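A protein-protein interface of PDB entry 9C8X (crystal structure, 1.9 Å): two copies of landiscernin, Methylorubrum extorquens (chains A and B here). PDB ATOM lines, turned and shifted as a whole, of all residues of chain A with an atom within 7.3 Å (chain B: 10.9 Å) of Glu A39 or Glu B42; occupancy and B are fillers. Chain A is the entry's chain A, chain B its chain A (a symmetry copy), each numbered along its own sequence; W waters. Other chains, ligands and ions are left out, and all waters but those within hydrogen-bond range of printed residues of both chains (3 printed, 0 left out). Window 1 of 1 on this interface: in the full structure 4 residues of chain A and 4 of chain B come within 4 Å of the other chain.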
ATOM      1  N   CYS A   6      14.094   0.359  19.443  1.00  0.00           N
ATOM      2  CA  CYS A   6      13.668   0.334  18.055  1.00  0.00           C
ATOM      3  C   CYS A   6      13.662  -1.089  17.517  1.00  0.00           C
ATOM      4  O   CYS A   6      12.697  -1.515  16.870  1.00  0.00           O
ATOM      5  CB  CYS A   6      14.570   1.242  17.221  1.00  0.00           C
ATOM      6  SG  CYS A   6      14.382   1.007  15.439  1.00  0.00           S
ATOM      7  N   LEU A  33       5.579   0.469   9.313  1.00  0.00           N
ATOM      8  CA  LEU A  33       6.637  -0.489   9.612  1.00  0.00           C
ATOM      9  C   LEU A  33       7.858  -0.248   8.742  1.00  0.00           C
ATOM     10  O   LEU A  33       8.993  -0.368   9.212  1.00  0.00           O
ATOM     11  CB  LEU A  33       6.133  -1.913   9.393  1.00  0.00           C
ATOM     12  CG  LEU A  33       5.952  -2.810  10.600  1.00  0.00           C
ATOM     13  CD1 LEU A  33       5.824  -4.218  10.089  1.00  0.00           C
ATOM     14  CD2 LEU A  33       7.152  -2.658  11.517  1.00  0.00           C
ATOM     15  N   LYS A  34       7.646   0.075   7.462  1.00  0.00           N
ATOM     16  CA  LYS A  34       8.785   0.292   6.577  1.00  0.00           C
ATOM     17  C   LYS A  34       9.483   1.617   6.859  1.00  0.00           C
ATOM     18  O   LYS A  34      10.709   1.704   6.709  1.00  0.00           O
ATOM     19  CB  LYS A  34       8.350   0.203   5.123  1.00  0.00           C
ATOM     20  CG  LYS A  34       7.875  -1.178   4.769  1.00  0.00           C
ATOM     21  CD  LYS A  34       8.193  -1.528   3.351  1.00  0.00           C
ATOM     22  CE  LYS A  34       7.471  -0.625   2.405  1.00  0.00           C
ATOM     23  NZ  LYS A  34       7.270  -1.326   1.073  1.00  0.00           N
ATOM     24  N   ILE A  35       8.742   2.646   7.279  1.00  0.00           N
ATOM     25  CA  ILE A  35       9.389   3.892   7.686  1.00  0.00           C
ATOM     26  C   ILE A  35      10.224   3.678   8.944  1.00  0.00           C
ATOM     27  O   ILE A  35      11.337   4.211   9.067  1.00  0.00           O
ATOM     28  CB  ILE A  35       8.349   5.007   7.876  1.00  0.00           C
ATOM     29  CG1 ILE A  35       7.744   5.397   6.524  1.00  0.00           C
ATOM     30  CG2 ILE A  35       8.988   6.210   8.553  1.00  0.00           C
ATOM     31  CD1 ILE A  35       6.576   6.360   6.623  1.00  0.00           C
ATOM     32  N   ALA A  36       9.721   2.886   9.896  1.00  0.00           N
ATOM     33  CA  ALA A  36      10.525   2.590  11.076  1.00  0.00           C
ATOM     34  C   ALA A  36      11.806   1.869  10.682  1.00  0.00           C
ATOM     35  O   ALA A  36      12.890   2.242  11.140  1.00  0.00           O
ATOM     36  CB  ALA A  36       9.732   1.774  12.091  1.00  0.00           C
ATOM     37  N   GLU A  37      11.708   0.894   9.776  1.00  0.00           N
ATOM     38  CA  GLU A  37      12.890   0.156   9.332  1.00  0.00           C
ATOM     39  C   GLU A  37      13.858   1.047   8.561  1.00  0.00           C
ATOM     40  O   GLU A  37      15.076   0.932   8.732  1.00  0.00           O
ATOM     41  CB  GLU A  37      12.463  -1.054   8.494  1.00  0.00           C
ATOM     42  CG  GLU A  37      11.913  -2.168   9.365  1.00  0.00           C
ATOM     43  CD  GLU A  37      11.090  -3.210   8.621  1.00  0.00           C
ATOM     44  OE1 GLU A  37      11.071  -3.202   7.369  1.00  0.00           O
ATOM     45  OE2 GLU A  37      10.451  -4.043   9.313  1.00  0.00           O
ATOM     46  N   ARG A  38      13.341   1.941   7.715  1.00  0.00           N
ATOM     47  CA  ARG A  38      14.199   2.903   7.031  1.00  0.00           C
ATOM     48  C   ARG A  38      14.964   3.772   8.030  1.00  0.00           C
ATOM     49  O   ARG A  38      16.186   3.920   7.945  1.00  0.00           O
ATOM     50  CB  ARG A  38      13.359   3.774   6.103  1.00  0.00           C
ATOM     51  CG  ARG A  38      14.138   4.924   5.506  1.00  0.00           C
ATOM     52  CD  ARG A  38      13.249   5.904   4.757  1.00  0.00           C
ATOM     53  NE  ARG A  38      12.684   6.918   5.637  1.00  0.00           N
ATOM     54  CZ  ARG A  38      11.700   7.740   5.299  1.00  0.00           C
ATOM     55  NH1 ARG A  38      11.107   7.664   4.118  1.00  0.00           N
ATOM     56  NH2 ARG A  38      11.316   8.681   6.158  1.00  0.00           N
ATOM     57  N   GLU A  39      14.251   4.366   8.984  1.00  0.00           N
ATOM     58  CA  GLU A  39      14.910   5.210   9.964  1.00  0.00           C
ATOM     59  C   GLU A  39      15.879   4.404  10.813  1.00  0.00           C
ATOM     60  O   GLU A  39      16.940   4.910  11.191  1.00  0.00           O
ATOM     61  CB  GLU A  39      13.870   5.907  10.836  1.00  0.00           C
ATOM     62  CG  GLU A  39      13.055   6.942  10.091  1.00  0.00           C
ATOM     63  CD  GLU A  39      13.917   8.007   9.445  1.00  0.00           C
ATOM     64  OE1 GLU A  39      14.798   8.565  10.127  1.00  0.00           O
ATOM     65  OE2 GLU A  39      13.714   8.303   8.249  1.00  0.00           O
ATOM     66  N   GLN A  40      15.524   3.160  11.150  1.00  0.00           N
ATOM     67  CA  GLN A  40      16.480   2.288  11.827  1.00  0.00           C
ATOM     68  C   GLN A  40      17.742   2.143  10.994  1.00  0.00           C
ATOM     69  O   GLN A  40      18.859   2.285  11.503  1.00  0.00           O
ATOM     70  CB  GLN A  40      15.864   0.913  12.090  1.00  0.00           C
ATOM     71  CG  GLN A  40      16.816  -0.065  12.765  1.00  0.00           C
ATOM     72  CD  GLN A  40      16.319  -1.500  12.718  1.00  0.00           C
ATOM     73  OE1 GLN A  40      15.843  -1.976  11.686  1.00  0.00           O
ATOM     74  NE2 GLN A  40      16.404  -2.186  13.851  1.00  0.00           N
ATOM     75  N   GLY A  41      17.573   1.893   9.691  1.00  0.00           N
ATOM     76  CA  GLY A  41      18.720   1.664   8.829  1.00  0.00           C
ATOM     77  C   GLY A  41      19.590   2.888   8.672  1.00  0.00           C
ATOM     78  O   GLY A  41      20.778   2.768   8.366  1.00  0.00           O
ATOM     79  N   GLU A  42      19.015   4.072   8.891  1.00  0.00           N
ATOM     80  CA  GLU A  42      19.734   5.340   8.861  1.00  0.00           C
ATOM     81  C   GLU A  42      20.357   5.710  10.205  1.00  0.00           C
ATOM     82  O   GLU A  42      21.050   6.724  10.286  1.00  0.00           O
ATOM     83  CB  GLU A  42      18.794   6.467   8.400  1.00  0.00           C
ATOM     84  CG  GLU A  42      18.167   6.232   7.038  1.00  0.00           C
ATOM     85  CD  GLU A  42      17.167   7.299   6.618  1.00  0.00           C
ATOM     86  OE1 GLU A  42      16.790   8.194   7.420  1.00  0.00           O
ATOM     87  OE2 GLU A  42      16.729   7.225   5.451  1.00  0.00           O
ATOM     88  N   GLY A  43      20.131   4.926  11.255  1.00  0.00           N
ATOM     89  CA  GLY A  43      20.657   5.264  12.560  1.00  0.00           C
ATOM     90  C   GLY A  43      19.871   6.313  13.304  1.00  0.00           C
ATOM     91  O   GLY A  43      20.370   6.863  14.293  1.00  0.00           O
ATOM     92  N   GLU A  44      18.647   6.612  12.863  1.00  0.00           N
ATOM     93  CA  GLU A  44      17.766   7.546  13.565  1.00  0.00           C
ATOM     94  C   GLU A  44      16.755   6.729  14.363  1.00  0.00           C
ATOM     95  O   GLU A  44      15.592   6.572  13.994  1.00  0.00           O
ATOM     96  CB  GLU A  44      17.105   8.490  12.574  1.00  0.00           C
ATOM     97  CG  GLU A  44      18.109   9.061  11.562  1.00  0.00           C
ATOM     98  CD  GLU A  44      17.576  10.263  10.831  1.00  0.00           C
ATOM     99  OE1 GLU A  44      17.267  11.268  11.502  1.00  0.00           O
ATOM    100  OE2 GLU A  44      17.434  10.202   9.594  1.00  0.00           O
ATOM    101  N   PHE A  45      17.235   6.172  15.470  1.00  0.00           N
ATOM    102  CA  PHE A  45      16.441   5.242  16.252  1.00  0.00           C
ATOM    103  C   PHE A  45      15.312   5.941  16.995  1.00  0.00           C
ATOM    104  O   PHE A  45      14.308   5.302  17.327  1.00  0.00           O
ATOM    105  CB  PHE A  45      17.360   4.478  17.217  1.00  0.00           C
ATOM    106  CG  PHE A  45      18.553   3.834  16.537  1.00  0.00           C
ATOM    107  CD1 PHE A  45      18.384   2.765  15.665  1.00  0.00           C
ATOM    108  CD2 PHE A  45      19.843   4.302  16.759  1.00  0.00           C
ATOM    109  CE1 PHE A  45      19.484   2.171  15.031  1.00  0.00           C
ATOM    110  CE2 PHE A  45      20.938   3.713  16.117  1.00  0.00           C
ATOM    111  CZ  PHE A  45      20.758   2.653  15.259  1.00  0.00           C
ATOM    112  N   ASP A  46      15.442   7.243  17.234  1.00  0.00           N
ATOM    113  CA  ASP A  46      14.340   7.982  17.830  1.00  0.00           C
ATOM    114  C   ASP A  46      13.186   8.132  16.847  1.00  0.00           C
ATOM    115  O   ASP A  46      12.019   8.049  17.240  1.00  0.00           O
ATOM    116  CB  ASP A  46      14.834   9.343  18.326  1.00  0.00           C
ATOM    117  CG  ASP A  46      15.699  10.062  17.307  1.00  0.00           C
ATOM    118  OD1 ASP A  46      15.858   9.559  16.167  1.00  0.00           O
ATOM    119  OD2 ASP A  46      16.217  11.145  17.653  1.00  0.00           O
ATOM    120  N   GLU A  47      13.492   8.335  15.563  1.00  0.00           N
ATOM    121  CA  GLU A  47      12.424   8.429  14.575  1.00  0.00           C
ATOM    122  C   GLU A  47      11.791   7.063  14.317  1.00  0.00           C
ATOM    123  O   GLU A  47      10.579   6.989  14.072  1.00  0.00           O
ATOM    124  CB  GLU A  47      12.950   9.048  13.280  1.00  0.00           C
ATOM    125  CG  GLU A  47      13.346  10.514  13.436  1.00  0.00           C
ATOM    126  CD  GLU A  47      12.287  11.327  14.174  1.00  0.00           C
ATOM    127  OE1 GLU A  47      11.105  11.324  13.741  1.00  0.00           O
ATOM    128  OE2 GLU A  47      12.639  11.954  15.199  1.00  0.00           O
ATOM    129  N   CYS A  48      12.581   5.991  14.364  1.00  0.00           N
ATOM    130  CA  CYS A  48      12.009   4.647  14.308  1.00  0.00           C
ATOM    131  C   CYS A  48      10.956   4.456  15.406  1.00  0.00           C
ATOM    132  O   CYS A  48       9.866   3.926  15.157  1.00  0.00           O
ATOM    133  CB  CYS A  48      13.127   3.608  14.431  1.00  0.00           C
ATOM    134  SG  CYS A  48      12.599   1.918  14.846  1.00  0.00           S
ATOM    135  N   LEU A  49      11.264   4.894  16.631  1.00  0.00           N
ATOM    136  CA  LEU A  49      10.298   4.763  17.712  1.00  0.00           C
ATOM    137  C   LEU A  49       9.030   5.554  17.420  1.00  0.00           C
ATOM    138  O   LEU A  49       7.924   5.085  17.703  1.00  0.00           O
ATOM    139  CB  LEU A  49      10.917   5.190  19.040  1.00  0.00           C
ATOM    140  CG  LEU A  49      12.002   4.280  19.631  1.00  0.00           C
ATOM    141  CD1 LEU A  49      12.612   4.912  20.877  1.00  0.00           C
ATOM    142  CD2 LEU A  49      11.437   2.918  19.957  1.00  0.00           C
ATOM    143  N   ALA A  51       7.763   6.187  14.428  1.00  0.00           N
ATOM    144  CA  ALA A  51       7.006   5.494  13.390  1.00  0.00           C
ATOM    145  C   ALA A  51       6.348   4.237  13.932  1.00  0.00           C
ATOM    146  O   ALA A  51       5.290   3.835  13.442  1.00  0.00           O
ATOM    147  CB  ALA A  51       7.906   5.147  12.201  1.00  0.00           C
ATOM    148  N   LYS B   3      11.018  23.762   4.700  1.00  0.00           N
ATOM    149  CA  LYS B   3      11.127  23.246   3.340  1.00  0.00           C
ATOM    150  C   LYS B   3      11.825  24.255   2.437  1.00  0.00           C
ATOM    151  O   LYS B   3      12.711  23.896   1.652  1.00  0.00           O
ATOM    152  CB  LYS B   3       9.736  22.880   2.803  1.00  0.00           C
ATOM    153  CG  LYS B   3       9.726  22.416   1.347  1.00  0.00           C
ATOM    154  CD  LYS B   3       8.445  21.670   0.997  1.00  0.00           C
ATOM    155  CE  LYS B   3       8.417  21.284  -0.482  1.00  0.00           C
ATOM    156  NZ  LYS B   3       7.148  20.563  -0.831  1.00  0.00           N
ATOM    157  N   CYS B   6      15.565  24.553   3.440  1.00  0.00           N
ATOM    158  CA  CYS B   6      16.300  23.370   3.030  1.00  0.00           C
ATOM    159  C   CYS B   6      16.653  23.438   1.552  1.00  0.00           C
ATOM    160  O   CYS B   6      17.796  23.168   1.163  1.00  0.00           O
ATOM    161  CB  CYS B   6      15.486  22.118   3.353  1.00  0.00           C
ATOM    162  SG  CYS B   6      16.117  20.622   2.558  1.00  0.00           S
ATOM    163  N   ILE B  10      20.508  23.993   0.279  1.00  0.00           N
ATOM    164  CA  ILE B  10      21.199  23.090  -0.640  1.00  0.00           C
ATOM    165  C   ILE B  10      21.749  23.865  -1.834  1.00  0.00           C
ATOM    166  O   ILE B  10      22.887  23.654  -2.265  1.00  0.00           O
ATOM    167  CB  ILE B  10      20.257  21.961  -1.088  1.00  0.00           C
ATOM    168  CG1 ILE B  10      19.934  21.037   0.091  1.00  0.00           C
ATOM    169  CG2 ILE B  10      20.859  21.198  -2.278  1.00  0.00           C
ATOM    170  CD1 ILE B  10      18.767  20.123  -0.154  1.00  0.00           C
ATOM    171  N   LYS B  34      24.583  14.799   0.483  1.00  0.00           N
ATOM    172  CA  LYS B  34      23.661  13.734   0.105  1.00  0.00           C
ATOM    173  C   LYS B  34      22.719  13.364   1.243  1.00  0.00           C
ATOM    174  O   LYS B  34      21.563  13.002   0.986  1.00  0.00           O
ATOM    175  CB  LYS B  34      24.431  12.517  -0.384  1.00  0.00           C
ATOM    176  CG  LYS B  34      25.184  12.809  -1.651  1.00  0.00           C
ATOM    177  CD  LYS B  34      25.263  11.610  -2.539  1.00  0.00           C
ATOM    178  CE  LYS B  34      26.035  10.512  -1.884  1.00  0.00           C
ATOM    179  NZ  LYS B  34      26.647   9.608  -2.940  1.00  0.00           N
ATOM    180  N   ILE B  35      23.172  13.458   2.497  1.00  0.00           N
ATOM    181  CA  ILE B  35      22.261  13.240   3.619  1.00  0.00           C
ATOM    182  C   ILE B  35      21.201  14.335   3.672  1.00  0.00           C
ATOM    183  O   ILE B  35      20.021  14.065   3.940  1.00  0.00           O
ATOM    184  CB  ILE B  35      23.042  13.140   4.940  1.00  0.00           C
ATOM    185  CG1 ILE B  35      23.876  11.855   4.960  1.00  0.00           C
ATOM    186  CG2 ILE B  35      22.084  13.185   6.119  1.00  0.00           C
ATOM    187  CD1 ILE B  35      24.824  11.752   6.140  1.00  0.00           C
ATOM    188  N   ALA B  36      21.586  15.587   3.404  1.00  0.00           N
ATOM    189  CA  ALA B  36      20.587  16.647   3.362  1.00  0.00           C
ATOM    190  C   ALA B  36      19.561  16.371   2.272  1.00  0.00           C
ATOM    191  O   ALA B  36      18.356  16.471   2.519  1.00  0.00           O
ATOM    192  CB  ALA B  36      21.240  18.011   3.162  1.00  0.00           C
ATOM    193  N   GLU B  37      20.017  15.945   1.093  1.00  0.00           N
ATOM    194  CA  GLU B  37      19.101  15.646  -0.007  1.00  0.00           C
ATOM    195  C   GLU B  37      18.212  14.447   0.307  1.00  0.00           C
ATOM    196  O   GLU B  37      17.021  14.457  -0.021  1.00  0.00           O
ATOM    197  CB  GLU B  37      19.895  15.424  -1.299  1.00  0.00           C
ATOM    198  CG  GLU B  37      20.395  16.736  -1.877  1.00  0.00           C
ATOM    199  CD  GLU B  37      21.520  16.596  -2.892  1.00  0.00           C
ATOM    200  OE1 GLU B  37      21.828  15.459  -3.319  1.00  0.00           O
ATOM    201  OE2 GLU B  37      22.103  17.649  -3.257  1.00  0.00           O
ATOM    202  N   ARG B  38      18.765  13.412   0.941  1.00  0.00           N
ATOM    203  CA  ARG B  38      17.950  12.282   1.375  1.00  0.00           C
ATOM    204  C   ARG B  38      16.849  12.729   2.336  1.00  0.00           C
ATOM    205  O   ARG B  38      15.671  12.403   2.156  1.00  0.00           O
ATOM    206  CB  ARG B  38      18.837  11.230   2.036  1.00  0.00           C
ATOM    207  CG  ARG B  38      18.048  10.118   2.688  1.00  0.00           C
ATOM    208  CD  ARG B  38      18.922   9.195   3.522  1.00  0.00           C
ATOM    209  NE  ARG B  38      19.102   9.686   4.881  1.00  0.00           N
ATOM    210  CZ  ARG B  38      19.997   9.211   5.737  1.00  0.00           C
ATOM    211  NH1 ARG B  38      20.852   8.263   5.392  1.00  0.00           N
ATOM    212  NH2 ARG B  38      20.020   9.684   6.982  1.00  0.00           N
ATOM    213  N   GLU B  39      17.218  13.474   3.375  1.00  0.00           N
ATOM    214  CA  GLU B  39      16.226  13.931   4.331  1.00  0.00           C
ATOM    215  C   GLU B  39      15.225  14.865   3.672  1.00  0.00           C
ATOM    216  O   GLU B  39      14.040  14.845   4.017  1.00  0.00           O
ATOM    217  CB  GLU B  39      16.913  14.613   5.511  1.00  0.00           C
ATOM    218  CG  GLU B  39      17.707  13.659   6.378  1.00  0.00           C
ATOM    219  CD  GLU B  39      16.863  12.523   6.917  1.00  0.00           C
ATOM    220  OE1 GLU B  39      15.772  12.786   7.458  1.00  0.00           O
ATOM    221  OE2 GLU B  39      17.290  11.354   6.815  1.00  0.00           O
ATOM    222  N   GLN B  40      15.681  15.711   2.744  1.00  0.00           N
ATOM    223  CA  GLN B  40      14.742  16.517   1.968  1.00  0.00           C
ATOM    224  C   GLN B  40      13.747  15.621   1.251  1.00  0.00           C
ATOM    225  O   GLN B  40      12.534  15.853   1.298  1.00  0.00           O
ATOM    226  CB  GLN B  40      15.488  17.389   0.956  1.00  0.00           C
ATOM    227  CG  GLN B  40      14.569  18.235   0.083  1.00  0.00           C
ATOM    228  CD  GLN B  40      15.281  18.829  -1.120  1.00  0.00           C
ATOM    229  OE1 GLN B  40      16.052  18.153  -1.802  1.00  0.00           O
ATOM    230  NE2 GLN B  40      15.044  20.111  -1.365  1.00  0.00           N
ATOM    231  N   GLY B  41      14.251  14.562   0.607  1.00  0.00           N
ATOM    232  CA  GLY B  41      13.386  13.690  -0.169  1.00  0.00           C
ATOM    233  C   GLY B  41      12.396  12.934   0.684  1.00  0.00           C
ATOM    234  O   GLY B  41      11.345  12.518   0.192  1.00  0.00           O
ATOM    235  N   GLU B  42      12.712  12.761   1.969  1.00  0.00           N
ATOM    236  CA  GLU B  42      11.832  12.126   2.941  1.00  0.00           C
ATOM    237  C   GLU B  42      10.863  13.105   3.603  1.00  0.00           C
ATOM    238  O   GLU B  42      10.021  12.674   4.391  1.00  0.00           O
ATOM    239  CB  GLU B  42      12.664  11.416   4.021  1.00  0.00           C
ATOM    240  CG  GLU B  42      13.620  10.369   3.477  1.00  0.00           C
ATOM    241  CD  GLU B  42      14.511   9.728   4.529  1.00  0.00           C
ATOM    242  OE1 GLU B  42      14.546  10.164   5.710  1.00  0.00           O
ATOM    243  OE2 GLU B  42      15.214   8.766   4.155  1.00  0.00           O
ATOM    244  N   GLY B  43      10.959  14.399   3.312  1.00  0.00           N
ATOM    245  CA  GLY B  43      10.097  15.368   3.954  1.00  0.00           C
ATOM    246  C   GLY B  43      10.515  15.756   5.349  1.00  0.00           C
ATOM    247  O   GLY B  43       9.721  16.361   6.079  1.00  0.00           O
ATOM    248  N   GLU B  44      11.746  15.430   5.751  1.00  0.00           N
ATOM    249  CA  GLU B  44      12.284  15.841   7.049  1.00  0.00           C
ATOM    250  C   GLU B  44      13.196  17.041   6.821  1.00  0.00           C
ATOM    251  O   GLU B  44      14.423  16.949   6.820  1.00  0.00           O
ATOM    252  CB  GLU B  44      13.001  14.676   7.711  1.00  0.00           C
ATOM    253  CG  GLU B  44      12.183  13.378   7.642  1.00  0.00           C
ATOM    254  CD  GLU B  44      12.677  12.329   8.600  1.00  0.00           C
ATOM    255  OE1 GLU B  44      12.661  12.594   9.818  1.00  0.00           O
ATOM    256  OE2 GLU B  44      13.110  11.252   8.144  1.00  0.00           O
ATOM    257  N   PHE B  45      12.565  18.188   6.593  1.00  0.00           N
ATOM    258  CA  PHE B  45      13.291  19.385   6.207  1.00  0.00           C
ATOM    259  C   PHE B  45      14.093  19.962   7.364  1.00  0.00           C
ATOM    260  O   PHE B  45      15.079  20.670   7.134  1.00  0.00           O
ATOM    261  CB  PHE B  45      12.303  20.415   5.639  1.00  0.00           C
ATOM    262  CG  PHE B  45      11.417  19.863   4.539  1.00  0.00           C
ATOM    263  CD1 PHE B  45      11.948  19.515   3.302  1.00  0.00           C
ATOM    264  CD2 PHE B  45      10.054  19.681   4.742  1.00  0.00           C
ATOM    265  CE1 PHE B  45      11.132  19.001   2.286  1.00  0.00           C
ATOM    266  CE2 PHE B  45       9.243  19.157   3.728  1.00  0.00           C
ATOM    267  CZ  PHE B  45       9.781  18.821   2.508  1.00  0.00           C
ATOM    268  N   ASP B  46      13.710  19.651   8.599  1.00  0.00           N
ATOM    269  CA  ASP B  46      14.513  20.075   9.734  1.00  0.00           C
ATOM    270  C   ASP B  46      15.827  19.305   9.794  1.00  0.00           C
ATOM    271  O   ASP B  46      16.868  19.876  10.128  1.00  0.00           O
ATOM    272  CB  ASP B  46      13.712  19.917  11.029  1.00  0.00           C
ATOM    273  CG  ASP B  46      13.005  18.576  11.123  1.00  0.00           C
ATOM    274  OD1 ASP B  46      13.196  17.713  10.230  1.00  0.00           O
ATOM    275  OD2 ASP B  46      12.259  18.387  12.106  1.00  0.00           O
ATOM    276  N   GLU B  47      15.799  18.013   9.458  1.00  0.00           N
ATOM    277  CA  GLU B  47      17.039  17.246   9.444  1.00  0.00           C
ATOM    278  C   GLU B  47      17.920  17.644   8.262  1.00  0.00           C
ATOM    279  O   GLU B  47      19.152  17.640   8.391  1.00  0.00           O
ATOM    280  CB  GLU B  47      16.739  15.748   9.430  1.00  0.00           C
ATOM    281  CG  GLU B  47      16.093  15.255  10.724  1.00  0.00           C
ATOM    282  CD  GLU B  47      16.812  15.772  11.965  1.00  0.00           C
ATOM    283  OE1 GLU B  47      18.048  15.565  12.086  1.00  0.00           O
ATOM    284  OE2 GLU B  47      16.137  16.403  12.811  1.00  0.00           O
ATOM    285  N   CYS B  48      17.319  17.982   7.122  1.00  0.00           N
ATOM    286  CA  CYS B  48      18.090  18.545   6.016  1.00  0.00           C
ATOM    287  C   CYS B  48      18.876  19.780   6.472  1.00  0.00           C
ATOM    288  O   CYS B  48      20.063  19.931   6.157  1.00  0.00           O
ATOM    289  CB  CYS B  48      17.150  18.888   4.857  1.00  0.00           C
ATOM    290  SG  CYS B  48      17.824  20.007   3.591  1.00  0.00           S
ATOM    291  N   ALA B  51      21.898  18.716   8.442  1.00  0.00           N
ATOM    292  CA  ALA B  51      22.974  18.162   7.625  1.00  0.00           C
ATOM    293  C   ALA B  51      23.676  19.248   6.828  1.00  0.00           C
ATOM    294  O   ALA B  51      24.869  19.125   6.537  1.00  0.00           O
ATOM    295  CB  ALA B  51      22.440  17.079   6.685  1.00  0.00           C
HETATM  296  O   HOH W   1      14.978  11.870  10.573  1.00  0.00           O
HETATM  297  O   HOH W   2      21.966   8.341   8.279  1.00  0.00           O
HETATM  298  O   HOH W   3       9.355  10.079   4.942  1.00  0.00           O
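The guanidinium group (NE) of Arg A38 lies within salt-bridge range of the side-chain carboxylate (OE2) of Glu B42 (3.5 Å).
The side-chain carboxylate of Glu B44 sits close to the guanidinium group of Arg A38, 3.7 Å away.
OE2 of Glu A42 lies within salt-bridge range of NE of Arg B38, 3.5 Å away.
The side-chain carboxylate of Glu A44 sits close to the guanidinium group of Arg B38 (3.7 Å).
OE1 of Glu B42 sits close to OE2 of Glu A39, 3.3 Å away.
OE2 of Glu A39 sits close to OE2 of Glu B44.
OE2 of Glu B39 sits close to OE1 of Glu A42, at 3.3 Å.
The side-chain carboxylate of Glu A42 lies close to the side-chain carboxylate of Glu B42.
The side-chain carboxylate (OE2) of Glu B39 sits close to the side-chain carboxylate (OE2) of Glu A44.
The side-chain carboxylate of Glu A39 lies close to the guanidinium group of Arg A38 (3.1 Å).
The side-chain carboxylate (OE2) of Glu B39 lies close to the guanidinium group (NE) of Arg B38, at 3.1 Å.
The side-chain sulfur of Cys A6 forms a disulfide with the side-chain sulfur of Cys A48, 2.1 Å away.
The side-chain sulfur (SG) of Cys B6 forms a disulfide with the side-chain sulfur (SG) of Cys B48 (2.1 Å).
Of chain B, only Glu B42 and Glu B44 come within 4 Å of Arg A38.
Of chain B, only Glu B42 (3.3 Å) and Glu B44 (3.0 Å) come within 4 Å of Glu A39.
No residue of chain B comes within 4 Å of Gly A41.
No residue of chain B comes within 4 Å of Gly A43.
Of the printed residues of chain B, Glu A44 touches Arg B38 (3.7 Å) and Glu B39 (3.0 Å).
No residue of chain B comes within 4 Å of Phe A45.
Cys A48 touches none of the printed residues of chain B.
Printed residues of chain A within 4 Å of Arg B38: Glu A42 and Glu A44.
Of the printed residues of chain A, Glu B39 touches Glu A42 and Glu A44.
Gln B40 touches none of the printed residues of chain A.
No residue of chain A comes within 4 Å of Gly B41.
Glu B42 touches just these residues of chain A: Arg A38, Glu A39 and Glu A42.
Of the printed residues of chain A, Glu B44 touches Arg A38 (3.7 Å) and Glu A39 (3.0 Å).
Cys B48 touches none of the printed residues of chain A.
Of the 19 printed residues of chain A, 4 touch a printed residue of chain B.
Of the 19 printed residues of chain B, 4 touch a printed residue of chain A.
Among the printed residues, Asp or Glu carboxylates within 4 Å of a Lys or Arg side-chain nitrogen of the other chain: Arg A38 with Glu B42 (3.5 Å), Arg A38 with Glu B44 (3.7 Å), Glu A42 with Arg B38 (3.5 Å) and Glu A44 with Arg B38 (3.7 Å).
Arg A38 touches Glu B42, and with the chains exchanged Glu A42 touches Arg B38.
Arg A38 touches Glu B44, and with the chains exchanged Glu A44 touches Arg B38.
Glu A39 touches Glu B42, and with the chains exchanged Glu A42 touches Glu B39.
Glu A39 touches Glu B44, and with the chains exchanged Glu A44 touches Glu B39.
Positions printed for both chains: 6, 34, 35, 36, 37, 38, 39, 40, 41, 42, 43, 44, 45, 46, 47, 48 and 51.
Of the 9 pairs that touch across the chains among the printed residues, 9 have their exchanged pair printed and touching as well.
Water W1 lies within hydrogen-bond range of the side-chain carboxylate (OE1) of Glu A44 (2.5 Å) and the side-chain carboxylate (OE1) of Glu B44 (2.5 Å).
Water W3 bridges the guanidinium group (NH2) of Arg A38 (2.7 Å) and the backbone carbonyl oxygen (O) of Glu B42 (2.7 Å).
Water W2 bridges NH2 of Arg B38 (2.7 Å) and O of Glu A42 (2.7 Å).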
